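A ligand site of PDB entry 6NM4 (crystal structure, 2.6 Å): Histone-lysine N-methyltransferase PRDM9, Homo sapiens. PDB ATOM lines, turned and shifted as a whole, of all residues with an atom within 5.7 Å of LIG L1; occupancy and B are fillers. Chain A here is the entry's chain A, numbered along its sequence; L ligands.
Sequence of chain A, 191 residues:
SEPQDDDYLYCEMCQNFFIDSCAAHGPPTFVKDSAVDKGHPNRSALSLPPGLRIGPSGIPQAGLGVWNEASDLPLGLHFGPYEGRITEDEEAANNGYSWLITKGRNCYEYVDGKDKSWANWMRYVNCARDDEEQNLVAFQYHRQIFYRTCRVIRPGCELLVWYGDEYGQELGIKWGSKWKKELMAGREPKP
OH of Tyr 82 lies within hydrogen-bond range of O of Tyr 97.
The backbone NH (N) of Tyr 97 sits at hydrogen-bond distance from the side-chain amide oxygen (OD1) of Asn 95 (2.8 Å).
The backbone carbonyl oxygen of Ala 62 sits at hydrogen-bond distance from the side-chain amide nitrogen of Asn 126, 3.1 Å away.
The backbone carbonyl oxygen (O) of Leu 64 is in hydrogen-bond range of the side-chain amide nitrogen (ND2) of Asn 126 (3.3 Å).
The side-chain amide nitrogen (ND2) of Asn 126 is in hydrogen-bond range of the side-chain hydroxyl (OG) of Ser 57, 2.7 Å away.
The backbone carbonyl oxygen (O) of Gly 63 sits at hydrogen-bond distance from the backbone NH (N) of Ser 57, 2.9 Å away.
An oxygen (O2) of LIG L1 lies within hydrogen-bond range of the side-chain hydroxyl (OH) of Tyr 97.
The backbone carbonyl oxygen of Ala 62 is in hydrogen-bond range of a nitrogen (N1) of LIG L1.
The backbone NH (N) of Leu 64 is in hydrogen-bond range of an oxygen (O1) of LIG L1, 2.9 Å away.
A nitrogen (N1) of LIG L1 lies within hydrogen-bond range of the backbone carbonyl oxygen (O) of Leu 64, 2.7 Å away.
OD1 of Asn 126 lies within hydrogen-bond range of N1 of LIG L1 (2.8 Å).
A nitrogen (N3) of LIG L1 is in hydrogen-bond range of the backbone NH (N) of Cys 127, 3.3 Å away.
The backbone carbonyl oxygen (O) of Cys 127 is in hydrogen-bond range of a nitrogen (N4) of LIG L1 (3.1 Å).
SG of Cys 127 lies close to N5 of LG2 L2 (3.8 Å).
O of Gly 96 sits close to S1 of LIG L1, at 3.7 Å.
The backbone carbonyl oxygen of Arg 123 lies close to a sulfur (S1) of LIG L1 (3.5 Å).
Residues that only touch LIG L1: Val 125, Tyr 124 and Gly 63.
Hydrophobic or aromatic side chains within 4 Å of LIG L1: Ala 62, Leu 64 and Tyr 97.
Ten residues have an atom within 4 Å of LIG L1: Ala 62, Gly 63, Leu 64, Gly 96, Tyr 97, Arg 123, Tyr 124, Val 125, Asn 126 and Cys 127.
The nearest printed residue that does not touch LIG L1 is Arg 129 (4.04 Å).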
ATOM      1  N   SER A  57      -6.899 -23.360   1.486  1.00  0.00           N
ATOM      2  CA  SER A  57      -6.213 -22.609   2.532  1.00  0.00           C
ATOM      3  C   SER A  57      -5.418 -21.416   1.972  1.00  0.00           C
ATOM      4  O   SER A  57      -4.837 -21.503   0.900  1.00  0.00           O
ATOM      5  CB  SER A  57      -5.287 -23.529   3.337  1.00  0.00           C
ATOM      6  OG  SER A  57      -4.626 -22.795   4.361  1.00  0.00           O
ATOM      7  N   ILE A  59      -2.752 -20.672   3.293  1.00  0.00           N
ATOM      8  CA  ILE A  59      -1.398 -21.204   3.411  1.00  0.00           C
ATOM      9  C   ILE A  59      -1.078 -22.070   2.189  1.00  0.00           C
ATOM     10  O   ILE A  59      -1.708 -23.103   1.994  1.00  0.00           O
ATOM     11  CB  ILE A  59      -1.255 -22.050   4.682  1.00  0.00           C
ATOM     12  CG1 ILE A  59      -1.496 -21.161   5.916  1.00  0.00           C
ATOM     13  CG2 ILE A  59       0.113 -22.726   4.749  1.00  0.00           C
ATOM     14  CD1 ILE A  59      -1.728 -21.927   7.184  1.00  0.00           C
ATOM     15  N   PRO A  60      -0.098 -21.672   1.376  1.00  0.00           N
ATOM     16  CA  PRO A  60       0.182 -22.421   0.143  1.00  0.00           C
ATOM     17  C   PRO A  60       0.494 -23.901   0.366  1.00  0.00           C
ATOM     18  O   PRO A  60       1.061 -24.254   1.391  1.00  0.00           O
ATOM     19  CB  PRO A  60       1.402 -21.694  -0.439  1.00  0.00           C
ATOM     20  CG  PRO A  60       1.278 -20.311   0.090  1.00  0.00           C
ATOM     21  CD  PRO A  60       0.746 -20.465   1.478  1.00  0.00           C
ATOM     22  N   GLN A  61       0.131 -24.738  -0.598  1.00  0.00           N
ATOM     23  CA  GLN A  61       0.321 -26.203  -0.529  1.00  0.00           C
ATOM     24  C   GLN A  61      -0.193 -26.843   0.764  1.00  0.00           C
ATOM     25  O   GLN A  61       0.376 -27.834   1.214  1.00  0.00           O
ATOM     26  CB  GLN A  61       1.810 -26.579  -0.669  1.00  0.00           C
ATOM     27  CG  GLN A  61       2.380 -26.520  -2.083  1.00  0.00           C
ATOM     28  CD  GLN A  61       3.039 -25.196  -2.380  1.00  0.00           C
ATOM     29  OE1 GLN A  61       2.765 -24.585  -3.397  1.00  0.00           O
ATOM     30  NE2 GLN A  61       3.914 -24.732  -1.480  1.00  0.00           N
ATOM     31  N   ALA A  62      -1.262 -26.304   1.346  1.00  0.00           N
ATOM     32  CA  ALA A  62      -1.751 -26.855   2.611  1.00  0.00           C
ATOM     33  C   ALA A  62      -3.186 -27.352   2.540  1.00  0.00           C
ATOM     34  O   ALA A  62      -3.915 -27.316   3.522  1.00  0.00           O
ATOM     35  CB  ALA A  62      -1.598 -25.817   3.736  1.00  0.00           C
ATOM     36  N   GLY A  63      -3.588 -27.819   1.365  1.00  0.00           N
ATOM     37  CA  GLY A  63      -4.942 -28.304   1.135  1.00  0.00           C
ATOM     38  C   GLY A  63      -6.023 -27.307   1.547  1.00  0.00           C
ATOM     39  O   GLY A  63      -5.941 -26.103   1.262  1.00  0.00           O
ATOM     40  N   LEU A  64      -7.038 -27.845   2.213  1.00  0.00           N
ATOM     41  CA  LEU A  64      -8.210 -27.069   2.619  1.00  0.00           C
ATOM     42  C   LEU A  64      -8.017 -26.446   3.994  1.00  0.00           C
ATOM     43  O   LEU A  64      -7.173 -26.893   4.796  1.00  0.00           O
ATOM     44  CB  LEU A  64      -9.453 -27.951   2.640  1.00  0.00           C
ATOM     45  CG  LEU A  64      -9.854 -28.534   1.267  1.00  0.00           C
ATOM     46  CD1 LEU A  64     -10.706 -29.786   1.385  1.00  0.00           C
ATOM     47  CD2 LEU A  64     -10.513 -27.455   0.434  1.00  0.00           C
ATOM     48  N   GLY A  65      -8.814 -25.419   4.239  1.00  0.00           N
ATOM     49  CA  GLY A  65      -8.832 -24.709   5.507  1.00  0.00           C
ATOM     50  C   GLY A  65     -10.252 -24.316   5.862  1.00  0.00           C
ATOM     51  O   GLY A  65     -11.162 -24.594   5.112  1.00  0.00           O
ATOM     52  N   TYR A  82     -13.316 -32.017  19.120  1.00  0.00           N
ATOM     53  CA  TYR A  82     -12.745 -32.642  17.939  1.00  0.00           C
ATOM     54  C   TYR A  82     -13.239 -34.079  17.958  1.00  0.00           C
ATOM     55  O   TYR A  82     -13.006 -34.801  18.916  1.00  0.00           O
ATOM     56  CB  TYR A  82     -11.213 -32.570  17.981  1.00  0.00           C
ATOM     57  CG  TYR A  82     -10.481 -32.939  16.687  1.00  0.00           C
ATOM     58  CD1 TYR A  82     -10.109 -34.231  16.427  1.00  0.00           C
ATOM     59  CD2 TYR A  82     -10.129 -31.967  15.751  1.00  0.00           C
ATOM     60  CE1 TYR A  82      -9.424 -34.572  15.273  1.00  0.00           C
ATOM     61  CE2 TYR A  82      -9.426 -32.283  14.601  1.00  0.00           C
ATOM     62  CZ  TYR A  82      -9.079 -33.608  14.371  1.00  0.00           C
ATOM     63  OH  TYR A  82      -8.387 -33.984  13.245  1.00  0.00           O
ATOM     64  N   ASN A  95      -0.526 -38.921  11.341  1.00  0.00           N
ATOM     65  CA  ASN A  95      -1.205 -39.153  10.052  1.00  0.00           C
ATOM     66  C   ASN A  95      -1.807 -37.840   9.530  1.00  0.00           C
ATOM     67  O   ASN A  95      -2.441 -37.829   8.502  1.00  0.00           O
ATOM     68  CB  ASN A  95      -2.277 -40.243  10.150  1.00  0.00           C
ATOM     69  CG  ASN A  95      -3.527 -39.809  10.950  1.00  0.00           C
ATOM     70  OD1 ASN A  95      -3.581 -38.720  11.523  1.00  0.00           O
ATOM     71  ND2 ASN A  95      -4.527 -40.687  10.998  1.00  0.00           N
ATOM     72  N   GLY A  96      -1.609 -36.747  10.259  1.00  0.00           N
ATOM     73  CA  GLY A  96      -2.134 -35.443   9.889  1.00  0.00           C
ATOM     74  C   GLY A  96      -3.387 -35.027  10.646  1.00  0.00           C
ATOM     75  O   GLY A  96      -3.699 -33.842  10.688  1.00  0.00           O
ATOM     76  N   TYR A  97      -4.121 -35.968  11.252  1.00  0.00           N
ATOM     77  CA  TYR A  97      -5.475 -35.685  11.775  1.00  0.00           C
ATOM     78  C   TYR A  97      -5.703 -36.156  13.228  1.00  0.00           C
ATOM     79  O   TYR A  97      -6.859 -36.224  13.691  1.00  0.00           O
ATOM     80  CB  TYR A  97      -6.517 -36.297  10.829  1.00  0.00           C
ATOM     81  CG  TYR A  97      -6.432 -35.762   9.409  1.00  0.00           C
ATOM     82  CD1 TYR A  97      -5.571 -36.352   8.489  1.00  0.00           C
ATOM     83  CD2 TYR A  97      -7.195 -34.692   8.996  1.00  0.00           C
ATOM     84  CE1 TYR A  97      -5.471 -35.882   7.185  1.00  0.00           C
ATOM     85  CE2 TYR A  97      -7.122 -34.204   7.701  1.00  0.00           C
ATOM     86  CZ  TYR A  97      -6.242 -34.808   6.801  1.00  0.00           C
ATOM     87  OH  TYR A  97      -6.138 -34.342   5.507  1.00  0.00           O
ATOM     88  N   MET A 122     -13.631 -29.823  12.262  1.00  0.00           N
ATOM     89  CA  MET A 122     -12.387 -29.290  12.811  1.00  0.00           C
ATOM     90  C   MET A 122     -11.171 -29.977  12.215  1.00  0.00           C
ATOM     91  O   MET A 122     -10.066 -29.478  12.333  1.00  0.00           O
ATOM     92  CB  MET A 122     -12.384 -29.401  14.335  1.00  0.00           C
ATOM     93  CG  MET A 122     -13.299 -28.399  14.998  1.00  0.00           C
ATOM     94  SD  MET A 122     -13.691 -28.847  16.698  1.00  0.00           S
ATOM     95  CE  MET A 122     -12.124 -28.523  17.508  1.00  0.00           C
ATOM     96  N   ARG A 123     -11.373 -31.115  11.562  1.00  0.00           N
ATOM     97  CA  ARG A 123     -10.303 -31.773  10.828  1.00  0.00           C
ATOM     98  C   ARG A 123      -9.804 -30.902   9.662  1.00  0.00           C
ATOM     99  O   ARG A 123      -8.720 -31.107   9.161  1.00  0.00           O
ATOM    100  CB  ARG A 123     -10.777 -33.133  10.306  1.00  0.00           C
ATOM    101  CG  ARG A 123     -11.577 -33.046   9.017  1.00  0.00           C
ATOM    102  CD  ARG A 123     -12.157 -34.363   8.583  1.00  0.00           C
ATOM    103  NE  ARG A 123     -11.151 -35.350   8.221  1.00  0.00           N
ATOM    104  CZ  ARG A 123     -10.453 -35.368   7.083  1.00  0.00           C
ATOM    105  NH1 ARG A 123     -10.604 -34.427   6.181  1.00  0.00           N
ATOM    106  NH2 ARG A 123      -9.586 -36.328   6.863  1.00  0.00           N
ATOM    107  N   TYR A 124     -10.612 -29.958   9.209  1.00  0.00           N
ATOM    108  CA  TYR A 124     -10.236 -29.128   8.064  1.00  0.00           C
ATOM    109  C   TYR A 124      -9.494 -27.861   8.476  1.00  0.00           C
ATOM    110  O   TYR A 124      -9.020 -27.142   7.605  1.00  0.00           O
ATOM    111  CB  TYR A 124     -11.480 -28.777   7.210  1.00  0.00           C
ATOM    112  CG  TYR A 124     -12.055 -29.974   6.499  1.00  0.00           C
ATOM    113  CD1 TYR A 124     -11.319 -30.659   5.528  1.00  0.00           C
ATOM    114  CD2 TYR A 124     -13.356 -30.444   6.786  1.00  0.00           C
ATOM    115  CE1 TYR A 124     -11.844 -31.747   4.871  1.00  0.00           C
ATOM    116  CE2 TYR A 124     -13.881 -31.546   6.135  1.00  0.00           C
ATOM    117  CZ  TYR A 124     -13.132 -32.194   5.175  1.00  0.00           C
ATOM    118  OH  TYR A 124     -13.638 -33.296   4.539  1.00  0.00           O
ATOM    119  N   VAL A 125      -9.361 -27.593   9.779  1.00  0.00           N
ATOM    120  CA  VAL A 125      -8.645 -26.406  10.259  1.00  0.00           C
ATOM    121  C   VAL A 125      -7.136 -26.577  10.149  1.00  0.00           C
ATOM    122  O   VAL A 125      -6.557 -27.521  10.688  1.00  0.00           O
ATOM    123  CB  VAL A 125      -8.972 -26.085  11.737  1.00  0.00           C
ATOM    124  CG1 VAL A 125      -8.205 -24.859  12.213  1.00  0.00           C
ATOM    125  CG2 VAL A 125     -10.458 -25.867  11.918  1.00  0.00           C
ATOM    126  N   ASN A 126      -6.479 -25.662   9.469  1.00  0.00           N
ATOM    127  CA  ASN A 126      -5.004 -25.714   9.335  1.00  0.00           C
ATOM    128  C   ASN A 126      -4.252 -25.141  10.553  1.00  0.00           C
ATOM    129  O   ASN A 126      -4.825 -24.452  11.397  1.00  0.00           O
ATOM    130  CB  ASN A 126      -4.554 -24.961   8.075  1.00  0.00           C
ATOM    131  CG  ASN A 126      -4.586 -25.830   6.836  1.00  0.00           C
ATOM    132  OD1 ASN A 126      -4.596 -27.065   6.897  1.00  0.00           O
ATOM    133  ND2 ASN A 126      -4.563 -25.172   5.690  1.00  0.00           N
ATOM    134  N   CYS A 127      -2.948 -25.415  10.612  1.00  0.00           N
ATOM    135  CA  CYS A 127      -2.132 -24.892  11.708  1.00  0.00           C
ATOM    136  C   CYS A 127      -1.487 -23.565  11.382  1.00  0.00           C
ATOM    137  O   CYS A 127      -0.964 -23.383  10.296  1.00  0.00           O
ATOM    138  CB  CYS A 127      -1.024 -25.867  12.065  1.00  0.00           C
ATOM    139  SG  CYS A 127      -1.675 -27.405  12.744  1.00  0.00           S
ATOM    140  N   ALA A 128      -1.527 -22.646  12.332  1.00  0.00           N
ATOM    141  CA  ALA A 128      -0.738 -21.417  12.255  1.00  0.00           C
ATOM    142  C   ALA A 128       0.738 -21.736  12.089  1.00  0.00           C
ATOM    143  O   ALA A 128       1.237 -22.745  12.608  1.00  0.00           O
ATOM    144  CB  ALA A 128      -0.939 -20.578  13.496  1.00  0.00           C
ATOM    145  N   ARG A 129       1.429 -20.867  11.338  1.00  0.00           N
ATOM    146  CA  ARG A 129       2.877 -20.964  11.170  1.00  0.00           C
ATOM    147  C   ARG A 129       3.632 -20.136  12.210  1.00  0.00           C
ATOM    148  O   ARG A 129       4.788 -20.405  12.490  1.00  0.00           O
ATOM    149  CB  ARG A 129       3.282 -20.508   9.777  1.00  0.00           C
ATOM    150  CG  ARG A 129       2.771 -21.432   8.693  1.00  0.00           C
ATOM    151  CD  ARG A 129       2.917 -20.823   7.318  1.00  0.00           C
ATOM    152  NE  ARG A 129       2.093 -19.623   7.158  1.00  0.00           N
ATOM    153  CZ  ARG A 129       1.918 -18.988   5.991  1.00  0.00           C
ATOM    154  NH1 ARG A 129       2.511 -19.418   4.870  1.00  0.00           N
ATOM    155  NH2 ARG A 129       1.147 -17.904   5.956  1.00  0.00           N
HETATM  156  N1  LIG L   1      -5.400 -28.947   4.941  1.00  0.00           N
HETATM  157  C1  LIG L   1      -5.894 -30.176   5.520  1.00  0.00           C
HETATM  158  C2  LIG L   1      -6.728 -30.934   4.523  1.00  0.00           C
HETATM  159  O1  LIG L   1      -6.960 -30.440   3.409  1.00  0.00           O
HETATM  160  O2  LIG L   1      -7.156 -32.058   4.839  1.00  0.00           O
HETATM  161  C3  LIG L   1      -6.681 -29.841   6.810  1.00  0.00           C
HETATM  162  C4  LIG L   1      -5.743 -29.714   7.999  1.00  0.00           C
HETATM  163  S1  LIG L   1      -5.240 -31.207   8.572  1.00  0.00           S
HETATM  164  C5  LIG L   1      -5.805 -31.350  10.134  1.00  0.00           C
HETATM  165  C6  LIG L   1      -3.575 -31.397   8.659  1.00  0.00           C
HETATM  166  C7  LIG L   1      -2.867 -31.600   7.323  1.00  0.00           C
HETATM  167  O3  LIG L   1      -2.970 -30.434   6.495  1.00  0.00           O
HETATM  168  C8  LIG L   1      -1.381 -31.881   7.514  1.00  0.00           C
HETATM  169  O4  LIG L   1      -1.043 -33.261   7.465  1.00  0.00           O
HETATM  170  C9  LIG L   1      -0.732 -31.204   6.335  1.00  0.00           C
HETATM  171  O5  LIG L   1      -0.654 -32.181   5.282  1.00  0.00           O
HETATM  172  C10 LIG L   1      -1.674 -30.045   6.052  1.00  0.00           C
HETATM  173  N2  LIG L   1      -1.310 -28.833   6.813  1.00  0.00           N
HETATM  174  C11 LIG L   1      -1.947 -28.323   7.908  1.00  0.00           C
HETATM  175  N3  LIG L   1      -1.348 -27.196   8.362  1.00  0.00           N
HETATM  176  C12 LIG L   1      -0.297 -26.973   7.531  1.00  0.00           C
HETATM  177  C13 LIG L   1       0.772 -25.960   7.433  1.00  0.00           C
HETATM  178  N4  LIG L   1       0.809 -24.949   8.322  1.00  0.00           N
HETATM  179  N5  LIG L   1       1.679 -26.084   6.429  1.00  0.00           N
HETATM  180  C14 LIG L   1       1.641 -27.082   5.535  1.00  0.00           C
HETATM  181  N6  LIG L   1       0.701 -28.047   5.576  1.00  0.00           N
HETATM  182  C15 LIG L   1      -0.266 -28.039   6.528  1.00  0.00           C
HETATM  183  C1  LG2 L   2      -0.067 -32.504  17.153  1.00  0.00           C
HETATM  184  C2  LG2 L   2       0.368 -31.071  13.849  1.00  0.00           C
HETATM  185  C3  LG2 L   2      -0.294 -30.747  12.673  1.00  0.00           C
HETATM  186  N1  LG2 L   2       3.261 -29.002  10.006  1.00  0.00           N
HETATM  187  C4  LG2 L   2       0.455 -30.141  11.536  1.00  0.00           C
HETATM  188  C5  LG2 L   2       2.072 -29.407  10.419  1.00  0.00           C
HETATM  189  N2  LG2 L   2       4.459 -25.656  13.814  1.00  0.00           N
HETATM  190  C6  LG2 L   2       4.325 -28.877  10.997  1.00  0.00           C
HETATM  191  C7  LG2 L   2       4.564 -27.374  11.368  1.00  0.00           C
HETATM  192  C8  LG2 L   2       3.280 -26.728  11.891  1.00  0.00           C
HETATM  193  C9  LG2 L   2       3.421 -25.502  12.790  1.00  0.00           C
HETATM  194  N3  LG2 L   2       4.792 -22.486  16.569  1.00  0.00           N
HETATM  195  C10 LG2 L   2       4.580 -24.597  14.737  1.00  0.00           C
HETATM  196  C11 LG2 L   2       3.651 -23.553  14.763  1.00  0.00           C
HETATM  197  C12 LG2 L   2       3.778 -22.518  15.684  1.00  0.00           C
HETATM  198  N4  LG2 L   2       5.145 -26.779  10.108  1.00  0.00           N
HETATM  199  C13 LG2 L   2       5.119 -25.323   9.918  1.00  0.00           C
HETATM  200  C14 LG2 L   2       5.614 -27.412  12.502  1.00  0.00           C
HETATM  201  C15 LG2 L   2       5.735 -26.075  13.212  1.00  0.00           C
HETATM  202  C16 LG2 L   2       5.618 -24.555  15.665  1.00  0.00           C
HETATM  203  C17 LG2 L   2       5.685 -23.485  16.545  1.00  0.00           C
HETATM  204  C18 LG2 L   2       2.804 -21.384  15.723  1.00  0.00           C
HETATM  205  C19 LG2 L   2       4.846 -27.501   8.851  1.00  0.00           C
HETATM  206  C20 LG2 L   2       3.424 -28.078   8.879  1.00  0.00           C
HETATM  207  O1  LG2 L   2       1.009 -29.397   9.598  1.00  0.00           O
HETATM  208  N5  LG2 L   2      -0.089 -29.898  10.377  1.00  0.00           N
HETATM  209  N6  LG2 L   2       1.796 -29.858  11.617  1.00  0.00           N
HETATM  210  C21 LG2 L   2      -0.310 -31.722  14.876  1.00  0.00           C
HETATM  211  O2  LG2 L   2       0.489 -31.905  15.977  1.00  0.00           O
HETATM  212  C22 LG2 L   2      -1.650 -32.063  14.731  1.00  0.00           C
HETATM  213  C23 LG2 L   2      -1.640 -31.063  12.530  1.00  0.00           C
HETATM  214  C24 LG2 L   2      -2.315 -31.706  13.559  1.00  0.00           C
HETATM  215  O3  LG2 L   2      -3.632 -31.872  13.262  1.00  0.00           O
HETATM  216  C25 LG2 L   2      -4.485 -32.480  14.242  1.00  0.00           C
